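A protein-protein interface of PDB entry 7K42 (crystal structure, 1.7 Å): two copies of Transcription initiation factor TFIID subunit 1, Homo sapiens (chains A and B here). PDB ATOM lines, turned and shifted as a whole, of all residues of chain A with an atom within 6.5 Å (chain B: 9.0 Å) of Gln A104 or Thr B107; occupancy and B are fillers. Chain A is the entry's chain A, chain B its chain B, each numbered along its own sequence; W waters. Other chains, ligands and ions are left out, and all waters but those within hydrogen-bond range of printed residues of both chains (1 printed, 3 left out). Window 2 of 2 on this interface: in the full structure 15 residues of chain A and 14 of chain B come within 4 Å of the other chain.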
ATOM      1  N   VAL A  99      14.171 -14.095 -18.521  1.00  0.00           N
ATOM      2  CA  VAL A  99      12.995 -14.855 -18.953  1.00  0.00           C
ATOM      3  C   VAL A  99      13.429 -16.145 -19.632  1.00  0.00           C
ATOM      4  O   VAL A  99      12.876 -17.223 -19.369  1.00  0.00           O
ATOM      5  CB  VAL A  99      12.112 -14.006 -19.892  1.00  0.00           C
ATOM      6  CG1 VAL A  99      11.028 -14.869 -20.545  1.00  0.00           C
ATOM      7  CG2 VAL A  99      11.467 -12.867 -19.138  1.00  0.00           C
ATOM      8  N   ASN A 100      14.431 -16.065 -20.507  1.00  0.00           N
ATOM      9  CA  ASN A 100      14.821 -17.239 -21.281  1.00  0.00           C
ATOM     10  C   ASN A 100      15.325 -18.369 -20.388  1.00  0.00           C
ATOM     11  O   ASN A 100      14.981 -19.540 -20.604  1.00  0.00           O
ATOM     12  CB  ASN A 100      15.900 -16.866 -22.299  1.00  0.00           C
ATOM     13  CG  ASN A 100      15.357 -16.074 -23.460  1.00  0.00           C
ATOM     14  OD1 ASN A 100      14.158 -16.108 -23.745  1.00  0.00           O
ATOM     15  ND2 ASN A 100      16.248 -15.371 -24.166  1.00  0.00           N
ATOM     16  N   VAL A 101      16.159 -18.055 -19.389  1.00  0.00           N
ATOM     17  CA  VAL A 101      16.663 -19.145 -18.557  1.00  0.00           C
ATOM     18  C   VAL A 101      15.533 -19.727 -17.719  1.00  0.00           C
ATOM     19  O   VAL A 101      15.527 -20.930 -17.421  1.00  0.00           O
ATOM     20  CB  VAL A 101      17.859 -18.689 -17.689  1.00  0.00           C
ATOM     21  CG1 VAL A 101      18.951 -18.096 -18.565  1.00  0.00           C
ATOM     22  CG2 VAL A 101      17.436 -17.697 -16.628  1.00  0.00           C
ATOM     23  N   CYS A 102      14.547 -18.904 -17.353  1.00  0.00           N
ATOM     24  CA  CYS A 102      13.380 -19.399 -16.629  1.00  0.00           C
ATOM     25  C   CYS A 102      12.537 -20.307 -17.514  1.00  0.00           C
ATOM     26  O   CYS A 102      12.250 -21.455 -17.160  1.00  0.00           O
ATOM     27  CB  CYS A 102      12.529 -18.227 -16.141  1.00  0.00           C
ATOM     28  SG  CYS A 102      11.000 -18.733 -15.328  1.00  0.00           S
ATOM     29  N   TYR A 103      12.137 -19.785 -18.673  1.00  0.00           N
ATOM     30  CA  TYR A 103      11.287 -20.520 -19.605  1.00  0.00           C
ATOM     31  C   TYR A 103      11.922 -21.842 -20.004  1.00  0.00           C
ATOM     32  O   TYR A 103      11.264 -22.893 -20.011  1.00  0.00           O
ATOM     33  CB  TYR A 103      11.049 -19.639 -20.836  1.00  0.00           C
ATOM     34  CG  TYR A 103      10.103 -20.206 -21.877  1.00  0.00           C
ATOM     35  CD1 TYR A 103      10.572 -21.025 -22.901  1.00  0.00           C
ATOM     36  CD2 TYR A 103       8.754 -19.914 -21.833  1.00  0.00           C
ATOM     37  CE1 TYR A 103       9.703 -21.546 -23.856  1.00  0.00           C
ATOM     38  CE2 TYR A 103       7.883 -20.431 -22.775  1.00  0.00           C
ATOM     39  CZ  TYR A 103       8.359 -21.235 -23.784  1.00  0.00           C
ATOM     40  OH  TYR A 103       7.482 -21.746 -24.727  1.00  0.00           O
ATOM     41  N   GLN A 104      13.210 -21.810 -20.330  1.00  0.00           N
ATOM     42  CA  GLN A 104      13.865 -23.012 -20.823  1.00  0.00           C
ATOM     43  C   GLN A 104      14.083 -24.028 -19.708  1.00  0.00           C
ATOM     44  O   GLN A 104      14.058 -25.240 -19.970  1.00  0.00           O
ATOM     45  CB  GLN A 104      15.148 -22.615 -21.552  1.00  0.00           C
ATOM     46  CG  GLN A 104      14.758 -21.895 -22.866  1.00  0.00           C
ATOM     47  CD  GLN A 104      15.870 -21.120 -23.544  1.00  0.00           C
ATOM     48  OE1 GLN A 104      15.638 -20.030 -24.081  1.00  0.00           O
ATOM     49  NE2 GLN A 104      17.069 -21.684 -23.565  1.00  0.00           N
ATOM     50  N   THR A 105      14.295 -23.564 -18.471  1.00  0.00           N
ATOM     51  CA  THR A 105      14.392 -24.496 -17.351  1.00  0.00           C
ATOM     52  C   THR A 105      13.030 -25.116 -17.053  1.00  0.00           C
ATOM     53  O   THR A 105      12.934 -26.318 -16.781  1.00  0.00           O
ATOM     54  CB  THR A 105      14.954 -23.792 -16.109  1.00  0.00           C
ATOM     55  OG1 THR A 105      16.214 -23.190 -16.426  1.00  0.00           O
ATOM     56  CG2 THR A 105      15.171 -24.790 -14.965  1.00  0.00           C
ATOM     57  N   LEU A 106      11.957 -24.318 -17.136  1.00  0.00           N
ATOM     58  CA  LEU A 106      10.614 -24.876 -16.998  1.00  0.00           C
ATOM     59  C   LEU A 106      10.357 -25.950 -18.046  1.00  0.00           C
ATOM     60  O   LEU A 106       9.738 -26.981 -17.753  1.00  0.00           O
ATOM     61  CB  LEU A 106       9.562 -23.770 -17.107  1.00  0.00           C
ATOM     62  CG  LEU A 106       9.447 -22.784 -15.947  1.00  0.00           C
ATOM     63  CD1 LEU A 106       8.424 -21.715 -16.307  1.00  0.00           C
ATOM     64  CD2 LEU A 106       9.054 -23.483 -14.649  1.00  0.00           C
ATOM     65  N   THR A 107      10.831 -25.731 -19.274  1.00  0.00           N
ATOM     66  CA  THR A 107      10.683 -26.748 -20.314  1.00  0.00           C
ATOM     67  C   THR A 107      11.438 -28.016 -19.954  1.00  0.00           C
ATOM     68  O   THR A 107      10.916 -29.127 -20.110  1.00  0.00           O
ATOM     69  CB  THR A 107      11.198 -26.208 -21.644  1.00  0.00           C
ATOM     70  OG1 THR A 107      10.347 -25.150 -22.079  1.00  0.00           O
ATOM     71  CG2 THR A 107      11.226 -27.309 -22.712  1.00  0.00           C
ATOM     72  N   GLU A 108      12.667 -27.865 -19.460  1.00  0.00           N
ATOM     73  CA  GLU A 108      13.465 -29.023 -19.079  1.00  0.00           C
ATOM     74  C   GLU A 108      12.782 -29.848 -17.994  1.00  0.00           C
ATOM     75  O   GLU A 108      12.839 -31.083 -18.016  1.00  0.00           O
ATOM     76  CB  GLU A 108      14.842 -28.555 -18.609  1.00  0.00           C
ATOM     77  CG  GLU A 108      15.834 -29.672 -18.340  1.00  0.00           C
ATOM     78  CD  GLU A 108      17.181 -29.137 -17.898  1.00  0.00           C
ATOM     79  OE1 GLU A 108      17.312 -27.899 -17.779  1.00  0.00           O
ATOM     80  OE2 GLU A 108      18.103 -29.949 -17.672  1.00  0.00           O
ATOM     81  N   TYR A 109      12.100 -29.187 -17.060  1.00  0.00           N
ATOM     82  CA  TYR A 109      11.462 -29.843 -15.926  1.00  0.00           C
ATOM     83  C   TYR A 109       9.998 -30.195 -16.176  1.00  0.00           C
ATOM     84  O   TYR A 109       9.271 -30.451 -15.207  1.00  0.00           O
ATOM     85  CB  TYR A 109      11.524 -28.953 -14.682  1.00  0.00           C
ATOM     86  CG  TYR A 109      12.886 -28.519 -14.161  1.00  0.00           C
ATOM     87  CD1 TYR A 109      14.074 -29.089 -14.623  1.00  0.00           C
ATOM     88  CD2 TYR A 109      12.968 -27.543 -13.167  1.00  0.00           C
ATOM     89  CE1 TYR A 109      15.307 -28.682 -14.112  1.00  0.00           C
ATOM     90  CE2 TYR A 109      14.188 -27.129 -12.652  1.00  0.00           C
ATOM     91  CZ  TYR A 109      15.354 -27.696 -13.123  1.00  0.00           C
ATOM     92  OH  TYR A 109      16.557 -27.263 -12.599  1.00  0.00           O
ATOM     93  N   ILE B  16      10.819 -22.573 -37.375  1.00  0.00           N
ATOM     94  CA  ILE B  16      10.595 -22.013 -36.043  1.00  0.00           C
ATOM     95  C   ILE B  16       9.280 -21.236 -36.020  1.00  0.00           C
ATOM     96  O   ILE B  16       8.480 -21.365 -35.086  1.00  0.00           O
ATOM     97  CB  ILE B  16      11.783 -21.137 -35.613  1.00  0.00           C
ATOM     98  CG1 ILE B  16      13.041 -21.994 -35.473  1.00  0.00           C
ATOM     99  CG2 ILE B  16      11.476 -20.434 -34.283  1.00  0.00           C
ATOM    100  CD1 ILE B  16      14.250 -21.192 -35.039  1.00  0.00           C
ATOM    101  N   ARG B  67      20.706 -14.685 -36.927  1.00  0.00           N
ATOM    102  CA  ARG B  67      19.595 -14.697 -35.978  1.00  0.00           C
ATOM    103  C   ARG B  67      19.260 -13.301 -35.475  1.00  0.00           C
ATOM    104  O   ARG B  67      18.114 -13.039 -35.094  1.00  0.00           O
ATOM    105  CB  ARG B  67      19.930 -15.591 -34.784  1.00  0.00           C
ATOM    106  CG  ARG B  67      19.794 -17.071 -35.052  1.00  0.00           C
ATOM    107  CD  ARG B  67      20.559 -17.882 -34.018  1.00  0.00           C
ATOM    108  NE  ARG B  67      21.978 -17.990 -34.351  1.00  0.00           N
ATOM    109  CZ  ARG B  67      22.853 -18.724 -33.670  1.00  0.00           C
ATOM    110  NH1 ARG B  67      24.124 -18.766 -34.050  1.00  0.00           N
ATOM    111  NH2 ARG B  67      22.461 -19.415 -32.607  1.00  0.00           N
ATOM    112  N   LEU B  71      15.573 -11.913 -34.869  1.00  0.00           N
ATOM    113  CA  LEU B  71      15.084 -11.597 -33.532  1.00  0.00           C
ATOM    114  C   LEU B  71      14.646 -10.148 -33.405  1.00  0.00           C
ATOM    115  O   LEU B  71      13.730  -9.851 -32.631  1.00  0.00           O
ATOM    116  CB  LEU B  71      16.159 -11.913 -32.496  1.00  0.00           C
ATOM    117  CG  LEU B  71      16.261 -13.382 -32.098  1.00  0.00           C
ATOM    118  CD1 LEU B  71      17.485 -13.578 -31.204  1.00  0.00           C
ATOM    119  CD2 LEU B  71      15.002 -13.825 -31.375  1.00  0.00           C
ATOM    120  N   VAL B  99       7.561 -15.036 -28.459  1.00  0.00           N
ATOM    121  CA  VAL B  99       8.970 -14.664 -28.364  1.00  0.00           C
ATOM    122  C   VAL B  99       9.746 -15.723 -27.591  1.00  0.00           C
ATOM    123  O   VAL B  99      10.861 -16.112 -27.978  1.00  0.00           O
ATOM    124  CB  VAL B  99       9.112 -13.273 -27.710  1.00  0.00           C
ATOM    125  CG1 VAL B  99      10.582 -12.954 -27.365  1.00  0.00           C
ATOM    126  CG2 VAL B  99       8.537 -12.205 -28.632  1.00  0.00           C
ATOM    127  N   ASN B 100       9.186 -16.187 -26.467  1.00  0.00           N
ATOM    128  CA  ASN B 100       9.937 -17.102 -25.607  1.00  0.00           C
ATOM    129  C   ASN B 100      10.195 -18.432 -26.297  1.00  0.00           C
ATOM    130  O   ASN B 100      11.290 -18.993 -26.179  1.00  0.00           O
ATOM    131  CB  ASN B 100       9.201 -17.323 -24.284  1.00  0.00           C
ATOM    132  CG  ASN B 100       9.193 -16.080 -23.407  1.00  0.00           C
ATOM    133  OD1 ASN B 100       9.938 -15.130 -23.648  1.00  0.00           O
ATOM    134  ND2 ASN B 100       8.332 -16.079 -22.390  1.00  0.00           N
ATOM    135  N   VAL B 101       9.192 -18.968 -27.000  1.00  0.00           N
ATOM    136  CA  VAL B 101       9.419 -20.242 -27.673  1.00  0.00           C
ATOM    137  C   VAL B 101      10.365 -20.050 -28.846  1.00  0.00           C
ATOM    138  O   VAL B 101      11.111 -20.968 -29.203  1.00  0.00           O
ATOM    139  CB  VAL B 101       8.088 -20.899 -28.102  1.00  0.00           C
ATOM    140  CG1 VAL B 101       7.511 -20.243 -29.365  1.00  0.00           C
ATOM    141  CG2 VAL B 101       8.309 -22.380 -28.360  1.00  0.00           C
ATOM    142  N   CYS B 102      10.385 -18.851 -29.434  1.00  0.00           N
ATOM    143  CA  CYS B 102      11.354 -18.554 -30.485  1.00  0.00           C
ATOM    144  C   CYS B 102      12.784 -18.639 -29.944  1.00  0.00           C
ATOM    145  O   CYS B 102      13.617 -19.374 -30.482  1.00  0.00           O
ATOM    146  CB  CYS B 102      11.064 -17.170 -31.071  1.00  0.00           C
ATOM    147  SG  CYS B 102      12.215 -16.650 -32.380  1.00  0.00           S
ATOM    148  N   TYR B 103      13.090 -17.892 -28.879  1.00  0.00           N
ATOM    149  CA  TYR B 103      14.424 -17.989 -28.272  1.00  0.00           C
ATOM    150  C   TYR B 103      14.768 -19.428 -27.906  1.00  0.00           C
ATOM    151  O   TYR B 103      15.894 -19.887 -28.137  1.00  0.00           O
ATOM    152  CB  TYR B 103      14.510 -17.111 -27.020  1.00  0.00           C
ATOM    153  CG  TYR B 103      14.852 -15.661 -27.303  1.00  0.00           C
ATOM    154  CD1 TYR B 103      16.176 -15.253 -27.439  1.00  0.00           C
ATOM    155  CD2 TYR B 103      13.848 -14.704 -27.433  1.00  0.00           C
ATOM    156  CE1 TYR B 103      16.492 -13.915 -27.688  1.00  0.00           C
ATOM    157  CE2 TYR B 103      14.154 -13.368 -27.683  1.00  0.00           C
ATOM    158  CZ  TYR B 103      15.478 -12.987 -27.805  1.00  0.00           C
ATOM    159  OH  TYR B 103      15.781 -11.670 -28.049  1.00  0.00           O
ATOM    160  N   GLN B 104      13.820 -20.155 -27.318  1.00  0.00           N
ATOM    161  CA  GLN B 104      14.128 -21.512 -26.887  1.00  0.00           C
ATOM    162  C   GLN B 104      14.476 -22.407 -28.066  1.00  0.00           C
ATOM    163  O   GLN B 104      15.394 -23.236 -27.984  1.00  0.00           O
ATOM    164  CB  GLN B 104      12.931 -22.101 -26.147  1.00  0.00           C
ATOM    165  CG  GLN B 104      13.065 -23.585 -25.887  1.00  0.00           C
ATOM    166  CD  GLN B 104      11.929 -24.103 -25.057  1.00  0.00           C
ATOM    167  OE1 GLN B 104      11.938 -23.978 -23.834  1.00  0.00           O
ATOM    168  NE2 GLN B 104      10.913 -24.663 -25.719  1.00  0.00           N
ATOM    169  N   THR B 105      13.773 -22.232 -29.187  1.00  0.00           N
ATOM    170  CA  THR B 105      14.037 -23.071 -30.350  1.00  0.00           C
ATOM    171  C   THR B 105      15.348 -22.680 -31.023  1.00  0.00           C
ATOM    172  O   THR B 105      16.096 -23.551 -31.480  1.00  0.00           O
ATOM    173  CB  THR B 105      12.858 -23.000 -31.323  1.00  0.00           C
ATOM    174  OG1 THR B 105      11.635 -23.185 -30.585  1.00  0.00           O
ATOM    175  CG2 THR B 105      12.972 -24.115 -32.336  1.00  0.00           C
ATOM    176  N   LEU B 106      15.644 -21.377 -31.092  1.00  0.00           N
ATOM    177  CA  LEU B 106      16.938 -20.943 -31.618  1.00  0.00           C
ATOM    178  C   LEU B 106      18.085 -21.540 -30.819  1.00  0.00           C
ATOM    179  O   LEU B 106      19.109 -21.951 -31.384  1.00  0.00           O
ATOM    180  CB  LEU B 106      17.038 -19.417 -31.591  1.00  0.00           C
ATOM    181  CG  LEU B 106      16.204 -18.645 -32.603  1.00  0.00           C
ATOM    182  CD1 LEU B 106      16.242 -17.158 -32.270  1.00  0.00           C
ATOM    183  CD2 LEU B 106      16.708 -18.895 -34.019  1.00  0.00           C
ATOM    184  N   THR B 107      17.933 -21.587 -29.497  1.00  0.00           N
ATOM    185  CA  THR B 107      18.960 -22.193 -28.661  1.00  0.00           C
ATOM    186  C   THR B 107      19.090 -23.676 -28.967  1.00  0.00           C
ATOM    187  O   THR B 107      20.205 -24.206 -29.060  1.00  0.00           O
ATOM    188  CB  THR B 107      18.624 -21.942 -27.195  1.00  0.00           C
ATOM    189  OG1 THR B 107      18.769 -20.542 -26.940  1.00  0.00           O
ATOM    190  CG2 THR B 107      19.540 -22.727 -26.282  1.00  0.00           C
ATOM    191  N   GLU B 108      17.959 -24.355 -29.147  1.00  0.00           N
ATOM    192  CA  GLU B 108      17.986 -25.766 -29.515  1.00  0.00           C
ATOM    193  C   GLU B 108      18.707 -25.990 -30.842  1.00  0.00           C
ATOM    194  O   GLU B 108      19.369 -27.018 -31.016  1.00  0.00           O
ATOM    195  CB  GLU B 108      16.552 -26.311 -29.554  1.00  0.00           C
ATOM    196  CG  GLU B 108      15.974 -26.525 -28.148  1.00  0.00           C
ATOM    197  CD  GLU B 108      14.453 -26.664 -28.087  1.00  0.00           C
ATOM    198  OE1 GLU B 108      13.930 -26.838 -26.960  1.00  0.00           O
ATOM    199  OE2 GLU B 108      13.783 -26.601 -29.140  1.00  0.00           O
ATOM    200  N   TYR B 109      18.586 -25.061 -31.794  1.00  0.00           N
ATOM    201  CA  TYR B 109      19.226 -25.200 -33.099  1.00  0.00           C
ATOM    202  C   TYR B 109      20.576 -24.484 -33.171  1.00  0.00           C
ATOM    203  O   TYR B 109      21.094 -24.275 -34.273  1.00  0.00           O
ATOM    204  CB  TYR B 109      18.309 -24.674 -34.209  1.00  0.00           C
ATOM    205  CG  TYR B 109      16.944 -25.340 -34.320  1.00  0.00           C
ATOM    206  CD1 TYR B 109      16.688 -26.581 -33.746  1.00  0.00           C
ATOM    207  CD2 TYR B 109      15.902 -24.706 -34.998  1.00  0.00           C
ATOM    208  CE1 TYR B 109      15.418 -27.175 -33.855  1.00  0.00           C
ATOM    209  CE2 TYR B 109      14.645 -25.286 -35.110  1.00  0.00           C
ATOM    210  CZ  TYR B 109      14.404 -26.518 -34.535  1.00  0.00           C
ATOM    211  OH  TYR B 109      13.152 -27.093 -34.643  1.00  0.00           O
ATOM    212  N   ASP B 110      21.160 -24.122 -32.023  1.00  0.00           N
ATOM    213  CA  ASP B 110      22.318 -23.226 -32.018  1.00  0.00           C
ATOM    214  C   ASP B 110      23.439 -23.759 -32.897  1.00  0.00           C
ATOM    215  O   ASP B 110      24.039 -23.008 -33.677  1.00  0.00           O
ATOM    216  CB  ASP B 110      22.817 -23.011 -30.591  1.00  0.00           C
ATOM    217  CG  ASP B 110      24.033 -22.087 -30.521  1.00  0.00           C
ATOM    218  OD1 ASP B 110      23.972 -20.953 -31.042  1.00  0.00           O
ATOM    219  OD2 ASP B 110      25.056 -22.487 -29.927  1.00  0.00           O
ATOM    220  N   GLU B 111      23.729 -25.056 -32.803  1.00  0.00           N
ATOM    221  CA  GLU B 111      24.897 -25.586 -33.499  1.00  0.00           C
ATOM    222  C   GLU B 111      24.708 -25.556 -35.011  1.00  0.00           C
ATOM    223  O   GLU B 111      25.643 -25.218 -35.747  1.00  0.00           O
ATOM    224  CB  GLU B 111      25.178 -27.003 -32.998  1.00  0.00           C
ATOM    225  CG  GLU B 111      26.396 -27.658 -33.597  1.00  0.00           C
ATOM    226  CD  GLU B 111      26.575 -29.078 -33.117  1.00  0.00           C
ATOM    227  OE1 GLU B 111      27.140 -29.906 -33.866  1.00  0.00           O
ATOM    228  OE2 GLU B 111      26.146 -29.378 -31.975  1.00  0.00           O
ATOM    229  N   HIS B 112      23.499 -25.869 -35.489  1.00  0.00           N
ATOM    230  CA  HIS B 112      23.202 -25.735 -36.912  1.00  0.00           C
ATOM    231  C   HIS B 112      23.277 -24.283 -37.361  1.00  0.00           C
ATOM    232  O   HIS B 112      23.892 -23.961 -38.387  1.00  0.00           O
ATOM    233  CB  HIS B 112      21.800 -26.266 -37.224  1.00  0.00           C
ATOM    234  CG  HIS B 112      21.705 -27.754 -37.345  1.00  0.00           C
ATOM    235  ND1 HIS B 112      21.954 -28.418 -38.526  1.00  0.00           N
ATOM    236  CD2 HIS B 112      21.325 -28.700 -36.454  1.00  0.00           C
ATOM    237  CE1 HIS B 112      21.772 -29.714 -38.347  1.00  0.00           C
ATOM    238  NE2 HIS B 112      21.386 -29.912 -37.100  1.00  0.00           N
ATOM    239  N   LEU B 113      22.639 -23.389 -36.602  1.00  0.00           N
ATOM    240  CA  LEU B 113      22.507 -22.005 -37.034  1.00  0.00           C
ATOM    241  C   LEU B 113      23.844 -21.280 -37.003  1.00  0.00           C
ATOM    242  O   LEU B 113      24.131 -20.464 -37.886  1.00  0.00           O
ATOM    243  CB  LEU B 113      21.478 -21.287 -36.161  1.00  0.00           C
ATOM    244  CG  LEU B 113      20.057 -21.843 -36.283  1.00  0.00           C
ATOM    245  CD1 LEU B 113      19.142 -21.147 -35.278  1.00  0.00           C
ATOM    246  CD2 LEU B 113      19.545 -21.669 -37.707  1.00  0.00           C
ATOM    247  N   THR B 114      24.680 -21.570 -36.005  1.00  0.00           N
ATOM    248  CA  THR B 114      25.990 -20.934 -35.958  1.00  0.00           C
ATOM    249  C   THR B 114      26.825 -21.309 -37.177  1.00  0.00           C
ATOM    250  O   THR B 114      27.473 -20.443 -37.776  1.00  0.00           O
ATOM    251  CB  THR B 114      26.717 -21.301 -34.661  1.00  0.00           C
ATOM    252  OG1 THR B 114      26.035 -20.701 -33.551  1.00  0.00           O
ATOM    253  CG2 THR B 114      28.157 -20.802 -34.697  1.00  0.00           C
HETATM  254  O   HOH W   1      17.607 -18.436 -25.537  1.00  0.00           O
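Of the 19 printed residues of chain B, 5 touch a printed residue of chain A. Along chain A the printed residues that touch a printed residue of chain B span positions 99 to 107. Among the printed residues, 9 pairs touch across the chains. Among the printed residues, no Asp or Glu carboxylate lies within 4 Å of a Lys or Arg side-chain nitrogen of the other chain.
The backbone carbonyl oxygen (O) of Tyr A103 is in hydrogen-bond range of the side-chain hydroxyl (OG1) of Thr A107 (3.2 Å). O of Val B101 sits at hydrogen-bond distance from OG1 of Thr B105. The backbone carbonyl oxygen (O) of Tyr B103 is in hydrogen-bond range of the side-chain hydroxyl (OG1) of Thr B107.
Water W1 lies within hydrogen-bond range of the side-chain hydroxyl of Thr B107, the side-chain amide oxygen of Gln A104 and the backbone carbonyl oxygen of Tyr B103.
Of chain B, only Tyr B103, Gln B104 and Thr B107 come within 4 Å of Gln A104. Of chain A, only Gln A104 comes within 4 Å of Thr B107. No residue of chain B comes within 4 Å of Thr A105. Of the printed residues of chain B, Asn A100 touches Tyr B103 (3.3 Å). Printed residues of chain B within 4 Å of Val A99: Asn B100. Of the printed residues of chain A, Tyr B103 touches Asn A100 and Gln A104. Printed residues of chain B within 4 Å of Tyr A103: Asn B100 (3.6 Å), Val B101 (3.5 Å) and Gln B104 (3.3 Å). Printed residues of chain A within 4 Å of Asn B100: Val A99 (3.3 Å) and Tyr A103 (3.6 Å). The nearest residue of chain A that does not touch Thr B107 is Asn A100 (6.4 Å). The nearest printed residue of chain A that does not touch Asn B100 is Asn A100 (4.3 Å).
The side-chain hydroxyl of Thr A107 lies within hydrogen-bond range of the side-chain amide oxygen of Gln B104 (2.6 Å).
Val A99 touches Asn B100, but with the chains exchanged Asn A100 does not touch Val B99 (5.4 Å). Tyr A103 touches Gln B104, and with the chains exchanged Gln A104 touches Tyr B103. Gln A104 touches its own counterpart, Gln B104. Gln A104 touches Thr B107, and with the chains exchanged Thr A107 touches Gln B104. Positions printed for both chains: 99, 100, 101, 102, 103, 104, 105, 106, 107, 108 and 109. Of the 9 pairs that touch across the chains among the printed residues, 7 have their exchanged pair printed and touching as well.
Among the printed residues, pairs that only touch across the chains: Asn A100 with Tyr B103 (3.3 Å), Val A99 with Asn B100 (3.3 Å), Tyr A103 with Gln B104 (3.3 Å), Gln A104 with Gln B104 (3.5 Å), Tyr A103 with Val B101 (3.5 Å), Tyr A103 with Asn B100 (3.6 Å), Gln A104 with Thr B107 (3.8 Å) and Gln A104 with Tyr B103 (3.97 Å).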
